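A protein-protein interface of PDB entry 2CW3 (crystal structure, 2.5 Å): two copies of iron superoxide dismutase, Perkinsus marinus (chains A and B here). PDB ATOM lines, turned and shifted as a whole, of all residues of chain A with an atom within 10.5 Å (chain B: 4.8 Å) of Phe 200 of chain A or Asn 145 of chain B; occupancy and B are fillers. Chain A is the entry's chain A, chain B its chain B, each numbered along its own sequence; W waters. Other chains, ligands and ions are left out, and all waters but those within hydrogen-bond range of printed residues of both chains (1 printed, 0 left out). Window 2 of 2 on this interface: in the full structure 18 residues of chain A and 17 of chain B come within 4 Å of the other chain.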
ATOM      1  N   MET A 193       7.386  -9.785  21.209  1.00  0.00           N
ATOM      2  CA  MET A 193       6.694  -8.564  20.773  1.00  0.00           C
ATOM      3  C   MET A 193       7.483  -7.911  19.651  1.00  0.00           C
ATOM      4  O   MET A 193       6.933  -7.535  18.623  1.00  0.00           O
ATOM      5  CB  MET A 193       6.505  -7.578  21.926  1.00  0.00           C
ATOM      6  CG  MET A 193       5.606  -8.069  23.049  1.00  0.00           C
ATOM      7  SD  MET A 193       3.882  -8.254  22.534  1.00  0.00           S
ATOM      8  CE  MET A 193       3.669  -6.697  21.637  1.00  0.00           C
ATOM      9  N   ARG A 194       8.790  -7.808  19.849  1.00  0.00           N
ATOM     10  CA  ARG A 194       9.707  -7.361  18.825  1.00  0.00           C
ATOM     11  C   ARG A 194       9.546  -8.150  17.483  1.00  0.00           C
ATOM     12  O   ARG A 194       9.236  -7.565  16.426  1.00  0.00           O
ATOM     13  CB  ARG A 194      11.104  -7.511  19.384  1.00  0.00           C
ATOM     14  CG  ARG A 194      12.178  -6.879  18.556  1.00  0.00           C
ATOM     15  CD  ARG A 194      13.575  -7.130  19.123  1.00  0.00           C
ATOM     16  NE  ARG A 194      13.675  -7.231  20.593  1.00  0.00           N
ATOM     17  CZ  ARG A 194      13.355  -6.274  21.472  1.00  0.00           C
ATOM     18  NH1 ARG A 194      12.837  -5.118  21.068  1.00  0.00           N
ATOM     19  NH2 ARG A 194      13.530  -6.503  22.774  1.00  0.00           N
ATOM     20  N   LYS A 195       9.752  -9.465  17.532  1.00  0.00           N
ATOM     21  CA  LYS A 195       9.602 -10.306  16.358  1.00  0.00           C
ATOM     22  C   LYS A 195       8.154 -10.328  15.803  1.00  0.00           C
ATOM     23  O   LYS A 195       7.962 -10.476  14.604  1.00  0.00           O
ATOM     24  CB  LYS A 195      10.089 -11.723  16.660  1.00  0.00           C
ATOM     25  CG  LYS A 195       9.926 -12.688  15.523  1.00  0.00           C
ATOM     26  CD  LYS A 195      10.511 -14.042  15.846  1.00  0.00           C
ATOM     27  CE  LYS A 195      11.978 -14.059  15.561  1.00  0.00           C
ATOM     28  NZ  LYS A 195      12.255 -13.779  14.113  1.00  0.00           N
ATOM     29  N   ALA A 196       7.142 -10.167  16.656  1.00  0.00           N
ATOM     30  CA  ALA A 196       5.787 -10.404  16.192  1.00  0.00           C
ATOM     31  C   ALA A 196       5.177  -9.185  15.560  1.00  0.00           C
ATOM     32  O   ALA A 196       4.255  -9.293  14.755  1.00  0.00           O
ATOM     33  CB  ALA A 196       4.915 -10.930  17.306  1.00  0.00           C
ATOM     34  N   THR A 197       5.698  -8.020  15.917  1.00  0.00           N
ATOM     35  CA  THR A 197       5.232  -6.756  15.329  1.00  0.00           C
ATOM     36  C   THR A 197       5.933  -6.469  13.988  1.00  0.00           C
ATOM     37  O   THR A 197       5.321  -5.901  13.074  1.00  0.00           O
ATOM     38  CB  THR A 197       5.449  -5.577  16.283  1.00  0.00           C
ATOM     39  OG1 THR A 197       6.824  -5.574  16.670  1.00  0.00           O
ATOM     40  CG2 THR A 197       4.612  -5.744  17.553  1.00  0.00           C
ATOM     41  N   ALA A 198       7.194  -6.888  13.882  1.00  0.00           N
ATOM     42  CA  ALA A 198       8.016  -6.673  12.710  1.00  0.00           C
ATOM     43  C   ALA A 198       7.673  -7.603  11.565  1.00  0.00           C
ATOM     44  O   ALA A 198       7.986  -7.288  10.408  1.00  0.00           O
ATOM     45  CB  ALA A 198       9.498  -6.821  13.057  1.00  0.00           C
ATOM     46  N   LEU A 199       7.044  -8.744  11.860  1.00  0.00           N
ATOM     47  CA  LEU A 199       6.734  -9.682  10.783  1.00  0.00           C
ATOM     48  C   LEU A 199       5.941  -8.955   9.687  1.00  0.00           C
ATOM     49  O   LEU A 199       4.835  -8.446   9.924  1.00  0.00           O
ATOM     50  CB  LEU A 199       5.980 -10.913  11.272  1.00  0.00           C
ATOM     51  CG  LEU A 199       5.797 -11.994  10.192  1.00  0.00           C
ATOM     52  CD1 LEU A 199       5.389 -13.368  10.807  1.00  0.00           C
ATOM     53  CD2 LEU A 199       4.830 -11.575   9.055  1.00  0.00           C
ATOM     54  N   PHE A 200       6.524  -8.886   8.497  1.00  0.00           N
ATOM     55  CA  PHE A 200       5.918  -8.116   7.432  1.00  0.00           C
ATOM     56  C   PHE A 200       5.050  -8.990   6.574  1.00  0.00           C
ATOM     57  O   PHE A 200       5.520  -9.986   6.016  1.00  0.00           O
ATOM     58  CB  PHE A 200       6.985  -7.434   6.565  1.00  0.00           C
ATOM     59  CG  PHE A 200       6.424  -6.370   5.698  1.00  0.00           C
ATOM     60  CD1 PHE A 200       6.083  -5.134   6.231  1.00  0.00           C
ATOM     61  CD2 PHE A 200       6.184  -6.604   4.350  1.00  0.00           C
ATOM     62  CE1 PHE A 200       5.526  -4.136   5.416  1.00  0.00           C
ATOM     63  CE2 PHE A 200       5.618  -5.610   3.547  1.00  0.00           C
ATOM     64  CZ  PHE A 200       5.298  -4.379   4.081  1.00  0.00           C
ATOM     65  N   GLY A 201       3.791  -8.597   6.440  1.00  0.00           N
ATOM     66  CA  GLY A 201       2.835  -9.347   5.629  1.00  0.00           C
ATOM     67  C   GLY A 201       1.954 -10.290   6.438  1.00  0.00           C
ATOM     68  O   GLY A 201       1.705 -10.071   7.637  1.00  0.00           O
ATOM     69  N   SER A 202       1.468 -11.329   5.764  1.00  0.00           N
ATOM     70  CA  SER A 202       0.672 -12.372   6.403  1.00  0.00           C
ATOM     71  C   SER A 202       1.605 -13.471   6.888  1.00  0.00           C
ATOM     72  O   SER A 202       2.404 -14.014   6.100  1.00  0.00           O
ATOM     73  CB  SER A 202      -0.334 -12.937   5.406  1.00  0.00           C
ATOM     74  OG  SER A 202      -1.185 -11.915   4.911  1.00  0.00           O
ATOM     75  N   GLY A 203       1.523 -13.792   8.177  1.00  0.00           N
ATOM     76  CA  GLY A 203       2.390 -14.819   8.751  1.00  0.00           C
ATOM     77  C   GLY A 203       1.980 -15.312  10.111  1.00  0.00           C
ATOM     78  O   GLY A 203       0.867 -15.045  10.555  1.00  0.00           O
ATOM     79  N   TRP A 204       2.895 -16.028  10.761  1.00  0.00           N
ATOM     80  CA  TRP A 204       2.675 -16.710  12.044  1.00  0.00           C
ATOM     81  C   TRP A 204       3.938 -16.602  12.900  1.00  0.00           C
ATOM     82  O   TRP A 204       5.053 -16.615  12.370  1.00  0.00           O
ATOM     83  CB  TRP A 204       2.418 -18.199  11.822  1.00  0.00           C
ATOM     84  CG  TRP A 204       1.252 -18.487  10.941  1.00  0.00           C
ATOM     85  CD1 TRP A 204       1.220 -18.442   9.571  1.00  0.00           C
ATOM     86  CD2 TRP A 204      -0.058 -18.866  11.366  1.00  0.00           C
ATOM     87  NE1 TRP A 204      -0.039 -18.741   9.124  1.00  0.00           N
ATOM     88  CE2 TRP A 204      -0.845 -19.007  10.206  1.00  0.00           C
ATOM     89  CE3 TRP A 204      -0.655 -19.080  12.623  1.00  0.00           C
ATOM     90  CZ2 TRP A 204      -2.194 -19.369  10.263  1.00  0.00           C
ATOM     91  CZ3 TRP A 204      -1.989 -19.432  12.674  1.00  0.00           C
ATOM     92  CH2 TRP A 204      -2.743 -19.575  11.502  1.00  0.00           C
ATOM     93  N   ILE A 205       3.759 -16.538  14.219  1.00  0.00           N
ATOM     94  CA  ILE A 205       4.878 -16.521  15.165  1.00  0.00           C
ATOM     95  C   ILE A 205       4.827 -17.808  15.964  1.00  0.00           C
ATOM     96  O   ILE A 205       3.768 -18.193  16.443  1.00  0.00           O
ATOM     97  CB  ILE A 205       4.840 -15.284  16.076  1.00  0.00           C
ATOM     98  CG1 ILE A 205       4.657 -14.023  15.230  1.00  0.00           C
ATOM     99  CG2 ILE A 205       6.109 -15.171  16.908  1.00  0.00           C
ATOM    100  CD1 ILE A 205       5.904 -13.628  14.416  1.00  0.00           C
ATOM    101  N   GLY A 220       9.332 -16.737  12.987  1.00  0.00           N
ATOM    102  CA  GLY A 220       8.282 -16.207  12.140  1.00  0.00           C
ATOM    103  C   GLY A 220       8.226 -17.022  10.861  1.00  0.00           C
ATOM    104  O   GLY A 220       9.266 -17.422  10.348  1.00  0.00           O
ATOM    105  N   THR A 221       7.019 -17.297  10.367  1.00  0.00           N
ATOM    106  CA  THR A 221       6.829 -17.943   9.066  1.00  0.00           C
ATOM    107  C   THR A 221       5.805 -17.158   8.271  1.00  0.00           C
ATOM    108  O   THR A 221       4.915 -16.541   8.843  1.00  0.00           O
ATOM    109  CB  THR A 221       6.343 -19.401   9.175  1.00  0.00           C
ATOM    110  OG1 THR A 221       5.022 -19.445   9.756  1.00  0.00           O
ATOM    111  CG2 THR A 221       7.313 -20.235   9.998  1.00  0.00           C
ATOM    112  N   LYS A 222       5.935 -17.179   6.950  1.00  0.00           N
ATOM    113  CA  LYS A 222       5.014 -16.434   6.112  1.00  0.00           C
ATOM    114  C   LYS A 222       3.861 -17.249   5.544  1.00  0.00           C
ATOM    115  O   LYS A 222       3.970 -18.456   5.291  1.00  0.00           O
ATOM    116  CB  LYS A 222       5.760 -15.626   5.039  1.00  0.00           C
ATOM    117  CG  LYS A 222       6.584 -16.437   4.023  1.00  0.00           C
ATOM    118  CD  LYS A 222       5.707 -17.170   2.979  1.00  0.00           C
ATOM    119  CE  LYS A 222       6.504 -17.680   1.757  1.00  0.00           C
ATOM    120  NZ  LYS A 222       5.564 -18.325   0.751  1.00  0.00           N
ATOM    121  N   ASP A 223       2.740 -16.564   5.383  1.00  0.00           N
ATOM    122  CA  ASP A 223       1.545 -17.092   4.728  1.00  0.00           C
ATOM    123  C   ASP A 223       1.059 -18.374   5.367  1.00  0.00           C
ATOM    124  O   ASP A 223       0.461 -18.338   6.437  1.00  0.00           O
ATOM    125  CB  ASP A 223       1.757 -17.246   3.221  1.00  0.00           C
ATOM    126  CG  ASP A 223       2.328 -15.984   2.579  1.00  0.00           C
ATOM    127  OD1 ASP A 223       2.068 -14.863   3.076  1.00  0.00           O
ATOM    128  OD2 ASP A 223       3.052 -16.120   1.568  1.00  0.00           O
ATOM    129  N   ALA A 224       1.332 -19.505   4.731  1.00  0.00           N
ATOM    130  CA  ALA A 224       0.821 -20.770   5.214  1.00  0.00           C
ATOM    131  C   ALA A 224       1.944 -21.692   5.681  1.00  0.00           C
ATOM    132  O   ALA A 224       1.680 -22.835   6.082  1.00  0.00           O
ATOM    133  CB  ALA A 224      -0.015 -21.432   4.142  1.00  0.00           C
ATOM    134  N   VAL A 242      -0.700 -14.039  12.916  1.00  0.00           N
ATOM    135  CA  VAL A 242      -0.431 -12.637  12.669  1.00  0.00           C
ATOM    136  C   VAL A 242      -1.071 -12.095  11.355  1.00  0.00           C
ATOM    137  O   VAL A 242      -0.812 -10.954  10.933  1.00  0.00           O
ATOM    138  CB  VAL A 242       1.086 -12.346  12.852  1.00  0.00           C
ATOM    139  CG1 VAL A 242       1.554 -11.220  11.985  1.00  0.00           C
ATOM    140  CG2 VAL A 242       1.366 -12.028  14.287  1.00  0.00           C
ATOM    141  N   TRP A 243      -1.894 -12.918  10.708  1.00  0.00           N
ATOM    142  CA  TRP A 243      -2.687 -12.456   9.569  1.00  0.00           C
ATOM    143  C   TRP A 243      -3.619 -11.388  10.095  1.00  0.00           C
ATOM    144  O   TRP A 243      -4.127 -11.506  11.213  1.00  0.00           O
ATOM    145  CB  TRP A 243      -3.525 -13.592   8.989  1.00  0.00           C
ATOM    146  CG  TRP A 243      -2.780 -14.542   8.088  1.00  0.00           C
ATOM    147  CD1 TRP A 243      -1.683 -15.295   8.407  1.00  0.00           C
ATOM    148  CD2 TRP A 243      -3.105 -14.863   6.732  1.00  0.00           C
ATOM    149  NE1 TRP A 243      -1.307 -16.068   7.335  1.00  0.00           N
ATOM    150  CE2 TRP A 243      -2.160 -15.820   6.291  1.00  0.00           C
ATOM    151  CE3 TRP A 243      -4.105 -14.438   5.847  1.00  0.00           C
ATOM    152  CZ2 TRP A 243      -2.173 -16.344   5.000  1.00  0.00           C
ATOM    153  CZ3 TRP A 243      -4.132 -14.968   4.574  1.00  0.00           C
ATOM    154  CH2 TRP A 243      -3.170 -15.909   4.153  1.00  0.00           C
ATOM    155  N   GLU A 244      -3.840 -10.343   9.305  1.00  0.00           N
ATOM    156  CA  GLU A 244      -4.688  -9.250   9.745  1.00  0.00           C
ATOM    157  C   GLU A 244      -6.080  -9.716  10.138  1.00  0.00           C
ATOM    158  O   GLU A 244      -6.696  -9.120  11.011  1.00  0.00           O
ATOM    159  CB  GLU A 244      -4.763  -8.143   8.693  1.00  0.00           C
ATOM    160  CG  GLU A 244      -3.488  -7.300   8.590  1.00  0.00           C
ATOM    161  CD  GLU A 244      -3.506  -6.379   7.388  1.00  0.00           C
ATOM    162  OE1 GLU A 244      -2.958  -5.263   7.461  1.00  0.00           O
ATOM    163  OE2 GLU A 244      -4.092  -6.764   6.359  1.00  0.00           O
ATOM    164  N   TYR A 247      -6.891 -10.162  13.969  1.00  0.00           N
ATOM    165  CA  TYR A 247      -7.091  -9.046  14.921  1.00  0.00           C
ATOM    166  C   TYR A 247      -7.798  -7.797  14.414  1.00  0.00           C
ATOM    167  O   TYR A 247      -8.103  -6.913  15.216  1.00  0.00           O
ATOM    168  CB  TYR A 247      -5.749  -8.589  15.513  1.00  0.00           C
ATOM    169  CG  TYR A 247      -4.705  -8.184  14.489  1.00  0.00           C
ATOM    170  CD1 TYR A 247      -4.658  -6.886  13.979  1.00  0.00           C
ATOM    171  CD2 TYR A 247      -3.745  -9.093  14.055  1.00  0.00           C
ATOM    172  CE1 TYR A 247      -3.684  -6.515  13.042  1.00  0.00           C
ATOM    173  CE2 TYR A 247      -2.769  -8.737  13.123  1.00  0.00           C
ATOM    174  CZ  TYR A 247      -2.745  -7.458  12.622  1.00  0.00           C
ATOM    175  OH  TYR A 247      -1.786  -7.111  11.709  1.00  0.00           O
ATOM    176  N   ARG A 255      -1.476  -3.996  15.689  1.00  0.00           N
ATOM    177  CA  ARG A 255      -1.071  -5.381  15.919  1.00  0.00           C
ATOM    178  C   ARG A 255      -0.414  -5.564  17.312  1.00  0.00           C
ATOM    179  O   ARG A 255      -0.592  -6.589  17.961  1.00  0.00           O
ATOM    180  CB  ARG A 255      -0.129  -5.856  14.793  1.00  0.00           C
ATOM    181  CG  ARG A 255       0.105  -7.345  14.799  1.00  0.00           C
ATOM    182  CD  ARG A 255       1.310  -7.738  14.000  1.00  0.00           C
ATOM    183  NE  ARG A 255       1.077  -7.766  12.549  1.00  0.00           N
ATOM    184  CZ  ARG A 255       2.027  -8.009  11.652  1.00  0.00           C
ATOM    185  NH1 ARG A 255       3.269  -8.242  12.046  1.00  0.00           N
ATOM    186  NH2 ARG A 255       1.747  -8.008  10.365  1.00  0.00           N
ATOM    187  N   LEU A 259      -1.200  -8.363  20.108  1.00  0.00           N
ATOM    188  CA  LEU A 259      -0.079  -9.141  20.625  1.00  0.00           C
ATOM    189  C   LEU A 259       0.153  -9.077  22.184  1.00  0.00           C
ATOM    190  O   LEU A 259       0.253 -10.140  22.833  1.00  0.00           O
ATOM    191  CB  LEU A 259       1.173  -8.747  19.810  1.00  0.00           C
ATOM    192  CG  LEU A 259       1.578  -9.518  18.526  1.00  0.00           C
ATOM    193  CD1 LEU A 259       0.626 -10.604  18.112  1.00  0.00           C
ATOM    194  CD2 LEU A 259       1.840  -8.620  17.381  1.00  0.00           C
ATOM    195  N   TYR B 111       3.755   4.295   7.178  1.00  0.00           N
ATOM    196  CA  TYR B 111       4.972   3.829   6.511  1.00  0.00           C
ATOM    197  C   TYR B 111       5.952   4.952   6.183  1.00  0.00           C
ATOM    198  O   TYR B 111       7.139   4.693   5.975  1.00  0.00           O
ATOM    199  CB  TYR B 111       4.639   3.120   5.218  1.00  0.00           C
ATOM    200  CG  TYR B 111       3.981   1.759   5.351  1.00  0.00           C
ATOM    201  CD1 TYR B 111       4.674   0.655   5.875  1.00  0.00           C
ATOM    202  CD2 TYR B 111       2.666   1.562   4.890  1.00  0.00           C
ATOM    203  CE1 TYR B 111       4.043  -0.614   5.956  1.00  0.00           C
ATOM    204  CE2 TYR B 111       2.038   0.314   4.974  1.00  0.00           C
ATOM    205  CZ  TYR B 111       2.725  -0.760   5.499  1.00  0.00           C
ATOM    206  OH  TYR B 111       2.074  -1.968   5.554  1.00  0.00           O
ATOM    207  N   GLU B 141      15.805  -4.447   3.662  1.00  0.00           N
ATOM    208  CA  GLU B 141      14.451  -4.981   3.824  1.00  0.00           C
ATOM    209  C   GLU B 141      13.389  -3.981   4.279  1.00  0.00           C
ATOM    210  O   GLU B 141      12.293  -3.940   3.715  1.00  0.00           O
ATOM    211  CB  GLU B 141      14.471  -6.143   4.806  1.00  0.00           C
ATOM    212  CG  GLU B 141      13.211  -6.982   4.780  1.00  0.00           C
ATOM    213  CD  GLU B 141      13.357  -8.166   3.859  1.00  0.00           C
ATOM    214  OE1 GLU B 141      12.517  -9.099   3.956  1.00  0.00           O
ATOM    215  OE2 GLU B 141      14.322  -8.167   3.057  1.00  0.00           O
ATOM    216  N   ASN B 142      13.702  -3.203   5.313  1.00  0.00           N
ATOM    217  CA  ASN B 142      12.736  -2.261   5.861  1.00  0.00           C
ATOM    218  C   ASN B 142      12.529  -1.044   5.003  1.00  0.00           C
ATOM    219  O   ASN B 142      11.393  -0.618   4.805  1.00  0.00           O
ATOM    220  CB  ASN B 142      13.085  -1.864   7.286  1.00  0.00           C
ATOM    221  CG  ASN B 142      12.576  -2.863   8.272  1.00  0.00           C
ATOM    222  OD1 ASN B 142      12.743  -4.072   8.085  1.00  0.00           O
ATOM    223  ND2 ASN B 142      11.911  -2.377   9.315  1.00  0.00           N
ATOM    224  N   VAL B 143      13.624  -0.499   4.483  1.00  0.00           N
ATOM    225  CA  VAL B 143      13.552   0.603   3.532  1.00  0.00           C
ATOM    226  C   VAL B 143      12.627   0.183   2.386  1.00  0.00           C
ATOM    227  O   VAL B 143      11.681   0.896   2.065  1.00  0.00           O
ATOM    228  CB  VAL B 143      14.950   0.967   3.003  1.00  0.00           C
ATOM    229  CG1 VAL B 143      14.852   1.906   1.820  1.00  0.00           C
ATOM    230  CG2 VAL B 143      15.787   1.569   4.110  1.00  0.00           C
ATOM    231  N   PHE B 144      12.886  -0.989   1.804  1.00  0.00           N
ATOM    232  CA  PHE B 144      12.110  -1.452   0.667  1.00  0.00           C
ATOM    233  C   PHE B 144      10.618  -1.600   1.012  1.00  0.00           C
ATOM    234  O   PHE B 144       9.754  -1.013   0.335  1.00  0.00           O
ATOM    235  CB  PHE B 144      12.663  -2.757   0.085  1.00  0.00           C
ATOM    236  CG  PHE B 144      11.796  -3.328  -0.985  1.00  0.00           C
ATOM    237  CD1 PHE B 144      11.753  -2.734  -2.254  1.00  0.00           C
ATOM    238  CD2 PHE B 144      10.980  -4.413  -0.723  1.00  0.00           C
ATOM    239  CE1 PHE B 144      10.924  -3.235  -3.253  1.00  0.00           C
ATOM    240  CE2 PHE B 144      10.139  -4.933  -1.700  1.00  0.00           C
ATOM    241  CZ  PHE B 144      10.112  -4.340  -2.976  1.00  0.00           C
ATOM    242  N   ASN B 145      10.332  -2.375   2.063  1.00  0.00           N
ATOM    243  CA  ASN B 145       8.965  -2.678   2.430  1.00  0.00           C
ATOM    244  C   ASN B 145       8.157  -1.398   2.604  1.00  0.00           C
ATOM    245  O   ASN B 145       6.960  -1.339   2.257  1.00  0.00           O
ATOM    246  CB  ASN B 145       8.937  -3.473   3.723  1.00  0.00           C
ATOM    247  CG  ASN B 145       9.287  -4.935   3.523  1.00  0.00           C
ATOM    248  OD1 ASN B 145       9.211  -5.468   2.402  1.00  0.00           O
ATOM    249  ND2 ASN B 145       9.660  -5.605   4.618  1.00  0.00           N
ATOM    250  N   ALA B 146       8.822  -0.371   3.135  1.00  0.00           N
ATOM    251  CA  ALA B 146       8.157   0.871   3.460  1.00  0.00           C
ATOM    252  C   ALA B 146       7.931   1.679   2.190  1.00  0.00           C
ATOM    253  O   ALA B 146       6.800   2.128   1.923  1.00  0.00           O
ATOM    254  CB  ALA B 146       8.965   1.674   4.477  1.00  0.00           C
ATOM    255  N   ALA B 147       8.989   1.851   1.403  1.00  0.00           N
ATOM    256  CA  ALA B 147       8.903   2.717   0.242  1.00  0.00           C
ATOM    257  C   ALA B 147       7.940   2.124  -0.760  1.00  0.00           C
ATOM    258  O   ALA B 147       7.175   2.863  -1.364  1.00  0.00           O
ATOM    259  CB  ALA B 147      10.243   2.926  -0.383  1.00  0.00           C
ATOM    260  N   GLY B 148       7.989   0.798  -0.929  1.00  0.00           N
ATOM    261  CA  GLY B 148       7.063   0.068  -1.798  1.00  0.00           C
ATOM    262  C   GLY B 148       5.596   0.267  -1.421  1.00  0.00           C
ATOM    263  O   GLY B 148       4.726   0.414  -2.293  1.00  0.00           O
ATOM    264  N   GLN B 149       5.328   0.293  -0.114  1.00  0.00           N
ATOM    265  CA  GLN B 149       3.963   0.466   0.397  1.00  0.00           C
ATOM    266  C   GLN B 149       3.453   1.893   0.236  1.00  0.00           C
ATOM    267  O   GLN B 149       2.244   2.114   0.080  1.00  0.00           O
ATOM    268  CB  GLN B 149       3.856   0.024   1.852  1.00  0.00           C
ATOM    269  CG  GLN B 149       3.922  -1.495   2.083  1.00  0.00           C
ATOM    270  CD  GLN B 149       2.720  -2.250   1.518  1.00  0.00           C
ATOM    271  OE1 GLN B 149       1.815  -2.601   2.256  1.00  0.00           O
ATOM    272  NE2 GLN B 149       2.705  -2.487   0.201  1.00  0.00           N
ATOM    273  N   ASP B 223       3.122  -8.840  -0.973  1.00  0.00           N
ATOM    274  CA  ASP B 223       3.533  -7.899   0.080  1.00  0.00           C
ATOM    275  C   ASP B 223       3.719  -6.440  -0.362  1.00  0.00           C
ATOM    276  O   ASP B 223       2.746  -5.724  -0.658  1.00  0.00           O
ATOM    277  CB  ASP B 223       4.803  -8.378   0.773  1.00  0.00           C
ATOM    278  CG  ASP B 223       4.652  -9.725   1.414  1.00  0.00           C
ATOM    279  OD1 ASP B 223       3.538 -10.131   1.759  1.00  0.00           O
ATOM    280  OD2 ASP B 223       5.678 -10.383   1.598  1.00  0.00           O
ATOM    281  N   ALA B 224       4.965  -5.995  -0.395  1.00  0.00           N
ATOM    282  CA  ALA B 224       5.233  -4.625  -0.779  1.00  0.00           C
ATOM    283  C   ALA B 224       5.716  -4.500  -2.240  1.00  0.00           C
ATOM    284  O   ALA B 224       5.932  -3.390  -2.747  1.00  0.00           O
ATOM    285  CB  ALA B 224       6.213  -4.001   0.192  1.00  0.00           C
ATOM    286  N   TRP B 243      -4.473  -6.619   0.510  1.00  0.00           N
ATOM    287  CA  TRP B 243      -4.233  -6.878   1.935  1.00  0.00           C
ATOM    288  C   TRP B 243      -5.577  -6.858   2.645  1.00  0.00           C
ATOM    289  O   TRP B 243      -6.467  -6.080   2.281  1.00  0.00           O
ATOM    290  CB  TRP B 243      -3.380  -5.773   2.565  1.00  0.00           C
ATOM    291  CG  TRP B 243      -1.935  -5.822   2.240  1.00  0.00           C
ATOM    292  CD1 TRP B 243      -1.377  -5.828   0.998  1.00  0.00           C
ATOM    293  CD2 TRP B 243      -0.844  -5.822   3.183  1.00  0.00           C
ATOM    294  NE1 TRP B 243      -0.008  -5.867   1.108  1.00  0.00           N
ATOM    295  CE2 TRP B 243       0.348  -5.850   2.433  1.00  0.00           C
ATOM    296  CE3 TRP B 243      -0.766  -5.820   4.587  1.00  0.00           C
ATOM    297  CZ2 TRP B 243       1.620  -5.876   3.037  1.00  0.00           C
ATOM    298  CZ3 TRP B 243       0.495  -5.836   5.191  1.00  0.00           C
ATOM    299  CH2 TRP B 243       1.671  -5.875   4.413  1.00  0.00           C
HETATM  300  O   HOH W   1       1.544 -12.095   2.658  1.00  0.00           O
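The backbone carbonyl oxygen (O) of Gly 201 of chain A is in hydrogen-bond range of the guanidinium group (NH2) of Arg 255 of chain A (3.4 Å).
OE1 of Gln 149 of chain B sits at hydrogen-bond distance from OH of Tyr 111 of chain B (3.4 Å).
The backbone carbonyl oxygen of Glu 141 of chain B sits close to the side-chain amide nitrogen of Asn 145 of chain B (3.2 Å).
The side-chain amide nitrogen (NE2) of Gln 149 of chain B lies within hydrogen-bond range of the backbone carbonyl oxygen (O) of Asp 223 of chain B.
The backbone carbonyl oxygen (O) of Asp 223 of chain B sits at hydrogen-bond distance from the indole nitrogen (NE1) of Trp 243 of chain B (3.3 Å).
Among the printed residues, pairs that only touch across the chains: Phe 200 of chain A with Tyr 111 of chain B, Phe 200 of chain A with Asn 145 of chain B, Phe 200 of chain A with Gln 149 of chain B, Phe 200 of chain A with Ala 224 of chain B, Phe 200 of chain A with Trp 243 of chain B, Gly 201 of chain A with Trp 243 of chain B and Glu 244 of chain A with Trp 243 of chain B.
Of the printed residues of chain B, Phe 200 of chain A touches Tyr 111 (3.9 Å), Asn 145 (3.5 Å), Gln 149 (3.8 Å), Ala 224 (3.8 Å) and Trp 243 (3.9 Å).
Of chain A, only Phe 200 (3.5 Å) comes within 4 Å of Asn 145 of chain B.
No residue of chain A comes within 4 Å of Glu 141 of chain B.
Asn 142 of chain B touches none of the printed residues of chain A.
No residue of chain A comes within 4 Å of Phe 144 of chain B.
No residue of chain A comes within 4 Å of Ala 146 of chain B.
Gln 149 of chain B touches one residue of chain A.
Of chain A, only Phe 200 (3.8 Å) comes within 4 Å of Ala 224 of chain B.
Printed residues of chain B within 4 Å of Gly 201 of chain A: Trp 243.
Of the printed residues of chain A, Tyr 111 of chain B touches Phe 200.
The nearest printed residue of chain B that does not touch Phe 200 of chain A is Asp 223 of chain B (4.003 Å).
The nearest residue of chain A that does not touch Asn 145 of chain B is Ala 198 of chain A (6.3 Å).
The nearest printed residue of chain B that does not touch Glu 244 of chain A is Tyr 111 of chain B (6.3 Å).
Of the 13 printed residues of chain B, 5 touch a printed residue of chain A.
Of the 24 printed residues of chain A, 3 touch a printed residue of chain B.
Hydrophobic or aromatic side chains of chain A within 4 Å of the printed part of chain B: Phe 200.
Among the printed residues, no Asp or Glu carboxylate lies within 4 Å of a Lys or Arg side-chain nitrogen of the other chain.
3 positions are printed for both chains.
Of the 7 pairs that touch across the chains among the printed residues, none has its exchanged pair printed and touching as well.
Water W1 lies within hydrogen-bond range of OD1 of Asp 223 of chain A, OD1 of Asp 223 of chain B and N of Ser 202 of chain A.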
